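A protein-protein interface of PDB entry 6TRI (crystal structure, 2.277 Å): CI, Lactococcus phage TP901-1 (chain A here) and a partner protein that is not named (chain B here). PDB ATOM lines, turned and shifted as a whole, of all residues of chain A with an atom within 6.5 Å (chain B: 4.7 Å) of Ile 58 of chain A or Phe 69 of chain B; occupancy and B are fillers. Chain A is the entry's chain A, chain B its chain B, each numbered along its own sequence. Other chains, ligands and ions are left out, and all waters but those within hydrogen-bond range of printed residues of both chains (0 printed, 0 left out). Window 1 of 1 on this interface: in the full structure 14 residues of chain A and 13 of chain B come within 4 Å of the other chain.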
ATOM      1  N   THR A   5     -21.829  26.666   8.015  1.00  0.00           N
ATOM      2  CA  THR A   5     -21.069  26.241   6.843  1.00  0.00           C
ATOM      3  C   THR A   5     -19.643  25.841   7.204  1.00  0.00           C
ATOM      4  O   THR A   5     -19.069  24.930   6.600  1.00  0.00           O
ATOM      5  CB  THR A   5     -21.031  27.352   5.775  1.00  0.00           C
ATOM      6  OG1 THR A   5     -22.368  27.773   5.480  1.00  0.00           O
ATOM      7  CG2 THR A   5     -20.372  26.852   4.499  1.00  0.00           C
ATOM      8  N   TYR A  46     -13.442  30.837   5.116  1.00  0.00           N
ATOM      9  CA  TYR A  46     -14.699  30.119   5.316  1.00  0.00           C
ATOM     10  C   TYR A  46     -14.511  28.949   6.275  1.00  0.00           C
ATOM     11  O   TYR A  46     -15.326  28.732   7.173  1.00  0.00           O
ATOM     12  CB  TYR A  46     -15.259  29.612   3.983  1.00  0.00           C
ATOM     13  CG  TYR A  46     -15.706  30.703   3.035  1.00  0.00           C
ATOM     14  CD1 TYR A  46     -15.930  31.996   3.485  1.00  0.00           C
ATOM     15  CD2 TYR A  46     -15.912  30.434   1.688  1.00  0.00           C
ATOM     16  CE1 TYR A  46     -16.339  32.995   2.620  1.00  0.00           C
ATOM     17  CE2 TYR A  46     -16.322  31.425   0.814  1.00  0.00           C
ATOM     18  CZ  TYR A  46     -16.535  32.703   1.286  1.00  0.00           C
ATOM     19  OH  TYR A  46     -16.943  33.694   0.422  1.00  0.00           O
ATOM     20  N   SER A  52     -18.582  34.342   6.711  1.00  0.00           N
ATOM     21  CA  SER A  52     -19.581  33.398   6.223  1.00  0.00           C
ATOM     22  C   SER A  52     -19.836  33.617   4.736  1.00  0.00           C
ATOM     23  O   SER A  52     -20.124  34.736   4.311  1.00  0.00           O
ATOM     24  CB  SER A  52     -20.888  33.534   7.009  1.00  0.00           C
ATOM     25  OG  SER A  52     -20.683  33.294   8.390  1.00  0.00           O
ATOM     26  N   PRO A  53     -19.720  32.547   3.938  1.00  0.00           N
ATOM     27  CA  PRO A  53     -19.940  32.628   2.489  1.00  0.00           C
ATOM     28  C   PRO A  53     -21.363  33.063   2.141  1.00  0.00           C
ATOM     29  O   PRO A  53     -22.311  32.618   2.787  1.00  0.00           O
ATOM     30  CB  PRO A  53     -19.671  31.197   2.011  1.00  0.00           C
ATOM     31  CG  PRO A  53     -19.854  30.346   3.227  1.00  0.00           C
ATOM     32  CD  PRO A  53     -19.376  31.182   4.369  1.00  0.00           C
ATOM     33  N   ASP A  54     -21.505  33.929   1.140  1.00  0.00           N
ATOM     34  CA  ASP A  54     -22.823  34.387   0.715  1.00  0.00           C
ATOM     35  C   ASP A  54     -23.481  33.377  -0.220  1.00  0.00           C
ATOM     36  O   ASP A  54     -22.939  32.296  -0.460  1.00  0.00           O
ATOM     37  CB  ASP A  54     -22.735  35.766   0.041  1.00  0.00           C
ATOM     38  CG  ASP A  54     -21.700  35.825  -1.075  1.00  0.00           C
ATOM     39  OD1 ASP A  54     -21.409  34.782  -1.697  1.00  0.00           O
ATOM     40  OD2 ASP A  54     -21.180  36.930  -1.338  1.00  0.00           O
ATOM     41  N   GLN A  55     -24.651  33.742  -0.737  1.00  0.00           N
ATOM     42  CA  GLN A  55     -25.439  32.875  -1.610  1.00  0.00           C
ATOM     43  C   GLN A  55     -24.621  32.299  -2.766  1.00  0.00           C
ATOM     44  O   GLN A  55     -24.664  31.097  -3.026  1.00  0.00           O
ATOM     45  CB  GLN A  55     -26.640  33.652  -2.156  1.00  0.00           C
ATOM     46  CG  GLN A  55     -27.515  32.880  -3.125  1.00  0.00           C
ATOM     47  CD  GLN A  55     -28.584  33.756  -3.749  1.00  0.00           C
ATOM     48  OE1 GLN A  55     -28.414  34.969  -3.874  1.00  0.00           O
ATOM     49  NE2 GLN A  55     -29.695  33.145  -4.142  1.00  0.00           N
ATOM     50  N   ASN A  56     -23.871  33.162  -3.448  1.00  0.00           N
ATOM     51  CA  ASN A  56     -23.061  32.757  -4.593  1.00  0.00           C
ATOM     52  C   ASN A  56     -22.050  31.665  -4.259  1.00  0.00           C
ATOM     53  O   ASN A  56     -22.012  30.624  -4.917  1.00  0.00           O
ATOM     54  CB  ASN A  56     -22.326  33.967  -5.175  1.00  0.00           C
ATOM     55  CG  ASN A  56     -23.262  34.939  -5.867  1.00  0.00           C
ATOM     56  OD1 ASN A  56     -24.261  34.538  -6.463  1.00  0.00           O
ATOM     57  ND2 ASN A  56     -22.939  36.226  -5.795  1.00  0.00           N
ATOM     58  N   ARG A  57     -21.237  31.903  -3.235  1.00  0.00           N
ATOM     59  CA  ARG A  57     -20.187  30.962  -2.860  1.00  0.00           C
ATOM     60  C   ARG A  57     -20.755  29.658  -2.296  1.00  0.00           C
ATOM     61  O   ARG A  57     -20.152  28.596  -2.452  1.00  0.00           O
ATOM     62  CB  ARG A  57     -19.226  31.605  -1.855  1.00  0.00           C
ATOM     63  CG  ARG A  57     -17.939  32.136  -2.483  1.00  0.00           C
ATOM     64  CD  ARG A  57     -18.175  33.387  -3.320  1.00  0.00           C
ATOM     65  NE  ARG A  57     -18.168  34.600  -2.505  1.00  0.00           N
ATOM     66  CZ  ARG A  57     -18.337  35.827  -2.985  1.00  0.00           C
ATOM     67  NH1 ARG A  57     -18.532  36.015  -4.285  1.00  0.00           N
ATOM     68  NH2 ARG A  57     -18.314  36.869  -2.165  1.00  0.00           N
ATOM     69  N   ILE A  58     -21.910  29.738  -1.641  1.00  0.00           N
ATOM     70  CA  ILE A  58     -22.610  28.539  -1.186  1.00  0.00           C
ATOM     71  C   ILE A  58     -22.995  27.687  -2.387  1.00  0.00           C
ATOM     72  O   ILE A  58     -22.751  26.480  -2.418  1.00  0.00           O
ATOM     73  CB  ILE A  58     -23.881  28.879  -0.378  1.00  0.00           C
ATOM     74  CG1 ILE A  58     -23.517  29.529   0.957  1.00  0.00           C
ATOM     75  CG2 ILE A  58     -24.709  27.627  -0.133  1.00  0.00           C
ATOM     76  CD1 ILE A  58     -22.767  28.611   1.888  1.00  0.00           C
ATOM     77  N   TYR A  59     -23.597  28.335  -3.380  1.00  0.00           N
ATOM     78  CA  TYR A  59     -23.986  27.672  -4.616  1.00  0.00           C
ATOM     79  C   TYR A  59     -22.783  27.010  -5.280  1.00  0.00           C
ATOM     80  O   TYR A  59     -22.863  25.873  -5.737  1.00  0.00           O
ATOM     81  CB  TYR A  59     -24.636  28.677  -5.568  1.00  0.00           C
ATOM     82  CG  TYR A  59     -25.174  28.069  -6.841  1.00  0.00           C
ATOM     83  CD1 TYR A  59     -26.382  27.384  -6.847  1.00  0.00           C
ATOM     84  CD2 TYR A  59     -24.484  28.192  -8.041  1.00  0.00           C
ATOM     85  CE1 TYR A  59     -26.883  26.829  -8.007  1.00  0.00           C
ATOM     86  CE2 TYR A  59     -24.978  27.641  -9.209  1.00  0.00           C
ATOM     87  CZ  TYR A  59     -26.179  26.961  -9.186  1.00  0.00           C
ATOM     88  OH  TYR A  59     -26.682  26.405 -10.339  1.00  0.00           O
ATOM     89  N   LEU A  60     -21.665  27.728  -5.310  1.00  0.00           N
ATOM     90  CA  LEU A  60     -20.445  27.238  -5.940  1.00  0.00           C
ATOM     91  C   LEU A  60     -19.911  25.970  -5.278  1.00  0.00           C
ATOM     92  O   LEU A  60     -19.615  24.984  -5.953  1.00  0.00           O
ATOM     93  CB  LEU A  60     -19.368  28.323  -5.913  1.00  0.00           C
ATOM     94  CG  LEU A  60     -18.024  27.896  -6.497  1.00  0.00           C
ATOM     95  CD1 LEU A  60     -18.163  27.602  -7.982  1.00  0.00           C
ATOM     96  CD2 LEU A  60     -16.966  28.954  -6.249  1.00  0.00           C
ATOM     97  N   LEU A  61     -19.791  25.999  -3.956  1.00  0.00           N
ATOM     98  CA  LEU A  61     -19.234  24.873  -3.217  1.00  0.00           C
ATOM     99  C   LEU A  61     -20.196  23.689  -3.181  1.00  0.00           C
ATOM    100  O   LEU A  61     -19.768  22.536  -3.169  1.00  0.00           O
ATOM    101  CB  LEU A  61     -18.862  25.308  -1.798  1.00  0.00           C
ATOM    102  CG  LEU A  61     -17.764  26.377  -1.779  1.00  0.00           C
ATOM    103  CD1 LEU A  61     -17.615  27.023  -0.407  1.00  0.00           C
ATOM    104  CD2 LEU A  61     -16.448  25.770  -2.237  1.00  0.00           C
ATOM    105  N   ALA A  62     -21.494  23.976  -3.172  1.00  0.00           N
ATOM    106  CA  ALA A  62     -22.505  22.922  -3.186  1.00  0.00           C
ATOM    107  C   ALA A  62     -22.417  22.104  -4.465  1.00  0.00           C
ATOM    108  O   ALA A  62     -22.320  20.877  -4.420  1.00  0.00           O
ATOM    109  CB  ALA A  62     -23.896  23.512  -3.034  1.00  0.00           C
ATOM    110  N   LYS A  63     -22.449  22.790  -5.605  1.00  0.00           N
ATOM    111  CA  LYS A  63     -22.374  22.123  -6.901  1.00  0.00           C
ATOM    112  C   LYS A  63     -21.026  21.436  -7.088  1.00  0.00           C
ATOM    113  O   LYS A  63     -20.934  20.384  -7.721  1.00  0.00           O
ATOM    114  CB  LYS A  63     -22.617  23.120  -8.035  1.00  0.00           C
ATOM    115  CG  LYS A  63     -23.996  23.753  -8.015  1.00  0.00           C
ATOM    116  CD  LYS A  63     -25.077  22.687  -7.979  1.00  0.00           C
ATOM    117  CE  LYS A  63     -26.465  23.289  -8.101  1.00  0.00           C
ATOM    118  NZ  LYS A  63     -26.697  23.892  -9.443  1.00  0.00           N
ATOM    119  N   SER A  68     -26.288  19.250  -1.067  1.00  0.00           N
ATOM    120  CA  SER A  68     -27.390  20.192  -0.909  1.00  0.00           C
ATOM    121  C   SER A  68     -26.923  21.514  -0.314  1.00  0.00           C
ATOM    122  O   SER A  68     -26.158  21.529   0.652  1.00  0.00           O
ATOM    123  CB  SER A  68     -28.480  19.585  -0.025  1.00  0.00           C
ATOM    124  OG  SER A  68     -29.357  20.585   0.461  1.00  0.00           O
ATOM    125  N   GLU A  69     -27.390  22.618  -0.890  1.00  0.00           N
ATOM    126  CA  GLU A  69     -27.053  23.949  -0.392  1.00  0.00           C
ATOM    127  C   GLU A  69     -27.519  24.118   1.046  1.00  0.00           C
ATOM    128  O   GLU A  69     -26.824  24.712   1.868  1.00  0.00           O
ATOM    129  CB  GLU A  69     -27.678  25.041  -1.269  1.00  0.00           C
ATOM    130  CG  GLU A  69     -27.081  25.172  -2.664  1.00  0.00           C
ATOM    131  CD  GLU A  69     -27.620  24.143  -3.640  1.00  0.00           C
ATOM    132  OE1 GLU A  69     -28.512  23.358  -3.254  1.00  0.00           O
ATOM    133  OE2 GLU A  69     -27.153  24.124  -4.799  1.00  0.00           O
ATOM    134  N   ALA A  70     -28.703  23.594   1.340  1.00  0.00           N
ATOM    135  CA  ALA A  70     -29.266  23.668   2.682  1.00  0.00           C
ATOM    136  C   ALA A  70     -28.377  22.944   3.684  1.00  0.00           C
ATOM    137  O   ALA A  70     -28.188  23.405   4.807  1.00  0.00           O
ATOM    138  CB  ALA A  70     -30.669  23.088   2.700  1.00  0.00           C
ATOM    139  N   LEU A  72     -25.145  22.402   3.293  1.00  0.00           N
ATOM    140  CA  LEU A  72     -23.874  23.111   3.348  1.00  0.00           C
ATOM    141  C   LEU A  72     -23.959  24.338   4.251  1.00  0.00           C
ATOM    142  O   LEU A  72     -22.940  24.859   4.697  1.00  0.00           O
ATOM    143  CB  LEU A  72     -23.440  23.520   1.940  1.00  0.00           C
ATOM    144  CG  LEU A  72     -21.990  23.951   1.743  1.00  0.00           C
ATOM    145  CD1 LEU A  72     -21.048  22.837   2.166  1.00  0.00           C
ATOM    146  CD2 LEU A  72     -21.758  24.346   0.287  1.00  0.00           C
ATOM    147  N   MET A  73     -25.178  24.791   4.523  1.00  0.00           N
ATOM    148  CA  MET A  73     -25.380  25.956   5.374  1.00  0.00           C
ATOM    149  C   MET A  73     -25.576  25.565   6.835  1.00  0.00           C
ATOM    150  O   MET A  73     -25.665  26.429   7.707  1.00  0.00           O
ATOM    151  CB  MET A  73     -26.578  26.771   4.885  1.00  0.00           C
ATOM    152  CG  MET A  73     -26.377  27.407   3.521  1.00  0.00           C
ATOM    153  SD  MET A  73     -27.694  28.560   3.104  1.00  0.00           S
ATOM    154  CE  MET A  73     -29.129  27.514   3.329  1.00  0.00           C
ATOM    155  N   TYR B   5     -30.828  33.789 -10.210  1.00  0.00           N
ATOM    156  CA  TYR B   5     -31.684  32.925  -9.406  1.00  0.00           C
ATOM    157  C   TYR B   5     -33.161  33.217  -9.648  1.00  0.00           C
ATOM    158  O   TYR B   5     -33.584  34.372  -9.679  1.00  0.00           O
ATOM    159  CB  TYR B   5     -31.360  33.073  -7.918  1.00  0.00           C
ATOM    160  CG  TYR B   5     -29.915  32.794  -7.578  1.00  0.00           C
ATOM    161  CD1 TYR B   5     -29.456  31.492  -7.422  1.00  0.00           C
ATOM    162  CD2 TYR B   5     -29.009  33.833  -7.407  1.00  0.00           C
ATOM    163  CE1 TYR B   5     -28.132  31.233  -7.111  1.00  0.00           C
ATOM    164  CE2 TYR B   5     -27.686  33.585  -7.095  1.00  0.00           C
ATOM    165  CZ  TYR B   5     -27.252  32.285  -6.946  1.00  0.00           C
ATOM    166  OH  TYR B   5     -25.933  32.040  -6.636  1.00  0.00           O
ATOM    167  N   ILE B  50     -30.637  34.519   4.548  1.00  0.00           N
ATOM    168  CA  ILE B  50     -31.354  33.329   4.108  1.00  0.00           C
ATOM    169  C   ILE B  50     -31.917  32.571   5.308  1.00  0.00           C
ATOM    170  O   ILE B  50     -33.070  32.143   5.296  1.00  0.00           O
ATOM    171  CB  ILE B  50     -30.449  32.396   3.278  1.00  0.00           C
ATOM    172  CG1 ILE B  50     -30.007  33.099   1.990  1.00  0.00           C
ATOM    173  CG2 ILE B  50     -31.172  31.096   2.954  1.00  0.00           C
ATOM    174  CD1 ILE B  50     -29.184  32.227   1.066  1.00  0.00           C
ATOM    175  N   ILE B  64     -35.075  24.816   0.621  1.00  0.00           N
ATOM    176  CA  ILE B  64     -34.192  25.964   0.425  1.00  0.00           C
ATOM    177  C   ILE B  64     -33.494  26.004  -0.948  1.00  0.00           C
ATOM    178  O   ILE B  64     -33.398  27.078  -1.548  1.00  0.00           O
ATOM    179  CB  ILE B  64     -33.130  26.030   1.546  1.00  0.00           C
ATOM    180  CG1 ILE B  64     -33.789  26.452   2.858  1.00  0.00           C
ATOM    181  CG2 ILE B  64     -32.022  27.008   1.194  1.00  0.00           C
ATOM    182  CD1 ILE B  64     -32.824  26.571   4.005  1.00  0.00           C
ATOM    183  N   PRO B  65     -33.016  24.850  -1.464  1.00  0.00           N
ATOM    184  CA  PRO B  65     -32.445  24.916  -2.817  1.00  0.00           C
ATOM    185  C   PRO B  65     -33.427  25.403  -3.887  1.00  0.00           C
ATOM    186  O   PRO B  65     -33.004  25.972  -4.894  1.00  0.00           O
ATOM    187  CB  PRO B  65     -32.034  23.465  -3.090  1.00  0.00           C
ATOM    188  CG  PRO B  65     -31.754  22.907  -1.748  1.00  0.00           C
ATOM    189  CD  PRO B  65     -32.772  23.534  -0.842  1.00  0.00           C
ATOM    190  N   TYR B  67     -35.844  27.607  -3.309  1.00  0.00           N
ATOM    191  CA  TYR B  67     -36.243  28.978  -3.014  1.00  0.00           C
ATOM    192  C   TYR B  67     -35.143  29.997  -3.311  1.00  0.00           C
ATOM    193  O   TYR B  67     -35.427  31.097  -3.784  1.00  0.00           O
ATOM    194  CB  TYR B  67     -36.675  29.103  -1.551  1.00  0.00           C
ATOM    195  CG  TYR B  67     -38.095  28.659  -1.291  1.00  0.00           C
ATOM    196  CD1 TYR B  67     -39.168  29.405  -1.754  1.00  0.00           C
ATOM    197  CD2 TYR B  67     -38.365  27.503  -0.571  1.00  0.00           C
ATOM    198  CE1 TYR B  67     -40.471  29.009  -1.521  1.00  0.00           C
ATOM    199  CE2 TYR B  67     -39.668  27.098  -0.329  1.00  0.00           C
ATOM    200  CZ  TYR B  67     -40.716  27.857  -0.808  1.00  0.00           C
ATOM    201  OH  TYR B  67     -42.015  27.466  -0.574  1.00  0.00           O
ATOM    202  N   PHE B  68     -33.894  29.633  -3.039  1.00  0.00           N
ATOM    203  CA  PHE B  68     -32.794  30.588  -3.134  1.00  0.00           C
ATOM    204  C   PHE B  68     -31.712  30.177  -4.130  1.00  0.00           C
ATOM    205  O   PHE B  68     -30.855  30.985  -4.484  1.00  0.00           O
ATOM    206  CB  PHE B  68     -32.156  30.793  -1.757  1.00  0.00           C
ATOM    207  CG  PHE B  68     -33.112  31.296  -0.713  1.00  0.00           C
ATOM    208  CD1 PHE B  68     -33.292  32.655  -0.518  1.00  0.00           C
ATOM    209  CD2 PHE B  68     -33.824  30.411   0.078  1.00  0.00           C
ATOM    210  CE1 PHE B  68     -34.172  33.123   0.442  1.00  0.00           C
ATOM    211  CE2 PHE B  68     -34.705  30.872   1.040  1.00  0.00           C
ATOM    212  CZ  PHE B  68     -34.879  32.228   1.221  1.00  0.00           C
ATOM    213  N   PHE B  69     -31.746  28.930  -4.586  1.00  0.00           N
ATOM    214  CA  PHE B  69     -30.670  28.429  -5.434  1.00  0.00           C
ATOM    215  C   PHE B  69     -31.177  27.804  -6.729  1.00  0.00           C
ATOM    216  O   PHE B  69     -30.587  26.856  -7.244  1.00  0.00           O
ATOM    217  CB  PHE B  69     -29.825  27.423  -4.652  1.00  0.00           C
ATOM    218  CG  PHE B  69     -29.264  27.979  -3.375  1.00  0.00           C
ATOM    219  CD1 PHE B  69     -28.059  28.661  -3.372  1.00  0.00           C
ATOM    220  CD2 PHE B  69     -29.952  27.838  -2.181  1.00  0.00           C
ATOM    221  CE1 PHE B  69     -27.543  29.182  -2.200  1.00  0.00           C
ATOM    222  CE2 PHE B  69     -29.444  28.359  -1.007  1.00  0.00           C
ATOM    223  CZ  PHE B  69     -28.237  29.032  -1.016  1.00  0.00           C
ATOM    224  N   ASN B  70     -32.265  28.354  -7.255  1.00  0.00           N
ATOM    225  CA  ASN B  70     -32.825  27.890  -8.516  1.00  0.00           C
ATOM    226  C   ASN B  70     -32.356  28.769  -9.670  1.00  0.00           C
ATOM    227  O   ASN B  70     -32.860  29.876  -9.863  1.00  0.00           O
ATOM    228  CB  ASN B  70     -34.355  27.866  -8.441  1.00  0.00           C
ATOM    229  CG  ASN B  70     -34.996  27.274  -9.681  1.00  0.00           C
ATOM    230  OD1 ASN B  70     -34.371  26.507 -10.412  1.00  0.00           O
ATOM    231  ND2 ASN B  70     -36.253  27.630  -9.923  1.00  0.00           N
ATOM    232  N   ALA B  71     -31.382  28.276 -10.427  1.00  0.00           N
ATOM    233  CA  ALA B  71     -30.839  29.019 -11.560  1.00  0.00           C
ATOM    234  C   ALA B  71     -31.869  29.171 -12.678  1.00  0.00           C
ATOM    235  O   ALA B  71     -32.648  28.256 -12.948  1.00  0.00           O
ATOM    236  CB  ALA B  71     -29.583  28.337 -12.084  1.00  0.00           C
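Of chain B, only Phe 69 (3.8 Å) comes within 4 Å of Ile 58 of chain A. Printed residues of chain B within 4 Å of Tyr 59 of chain A: Tyr 5 (3.8 Å), Phe 69 (3.8 Å) and Ala 71 (3.9 Å). Printed residues of chain B within 4 Å of Gln 55 of chain A: Tyr 5 (3.4 Å), Phe 68 (2.5 Å) and Phe 69 (3.6 Å). Pro 53 of chain A touches none of the printed residues of chain B.
CD2 of Tyr 5 of chain B touches NE2 of Gln 55 of chain A (3.4 Å). O of Gln 55 of chain A touches CE1 of Phe 69 of chain B, at 3.6 Å. Phe 69 of chain B touches Ile 58 of chain A (CE1 to CG2, 3.8 Å). CB of Tyr 59 of chain A touches OH of Tyr 5 of chain B, at 3.8 Å. Tyr 59 of chain A touches Phe 69 of chain B. Tyr 59 of chain A touches Ala 71 of chain B (OH to CB, 3.9 Å). Glu 69 of chain A touches Pro 65 of chain B. CG of Phe 69 of chain B touches CG of Glu 69 of chain A (3.6 Å). CE of Met 73 of chain A touches CG2 of Ile 64 of chain B, 3.6 Å away.
OD1 of Asp 54 of chain A lies close to N of Asn 56 of chain A. NZ of Lys 63 of chain A sits at hydrogen-bond distance from OH of Tyr 59 of chain A, 2.7 Å away. The backbone carbonyl oxygen (O) of Pro 65 of chain B is in hydrogen-bond range of the backbone NH (N) of Asn 70 of chain B, at 3.4 Å.
Printed residues of chain A that touch a printed residue of chain B: Gln 55, Asn 56, Ile 58, Tyr 59, Glu 69 and Met 73. Of the 9 printed residues of chain B, 6 touch a printed residue of chain A.
NE2 of Gln 55 of chain A sits at hydrogen-bond distance from O of Phe 68 of chain B (2.5 Å). OD1 of Asn 56 of chain A sits at hydrogen-bond distance from OH of Tyr 5 of chain B.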
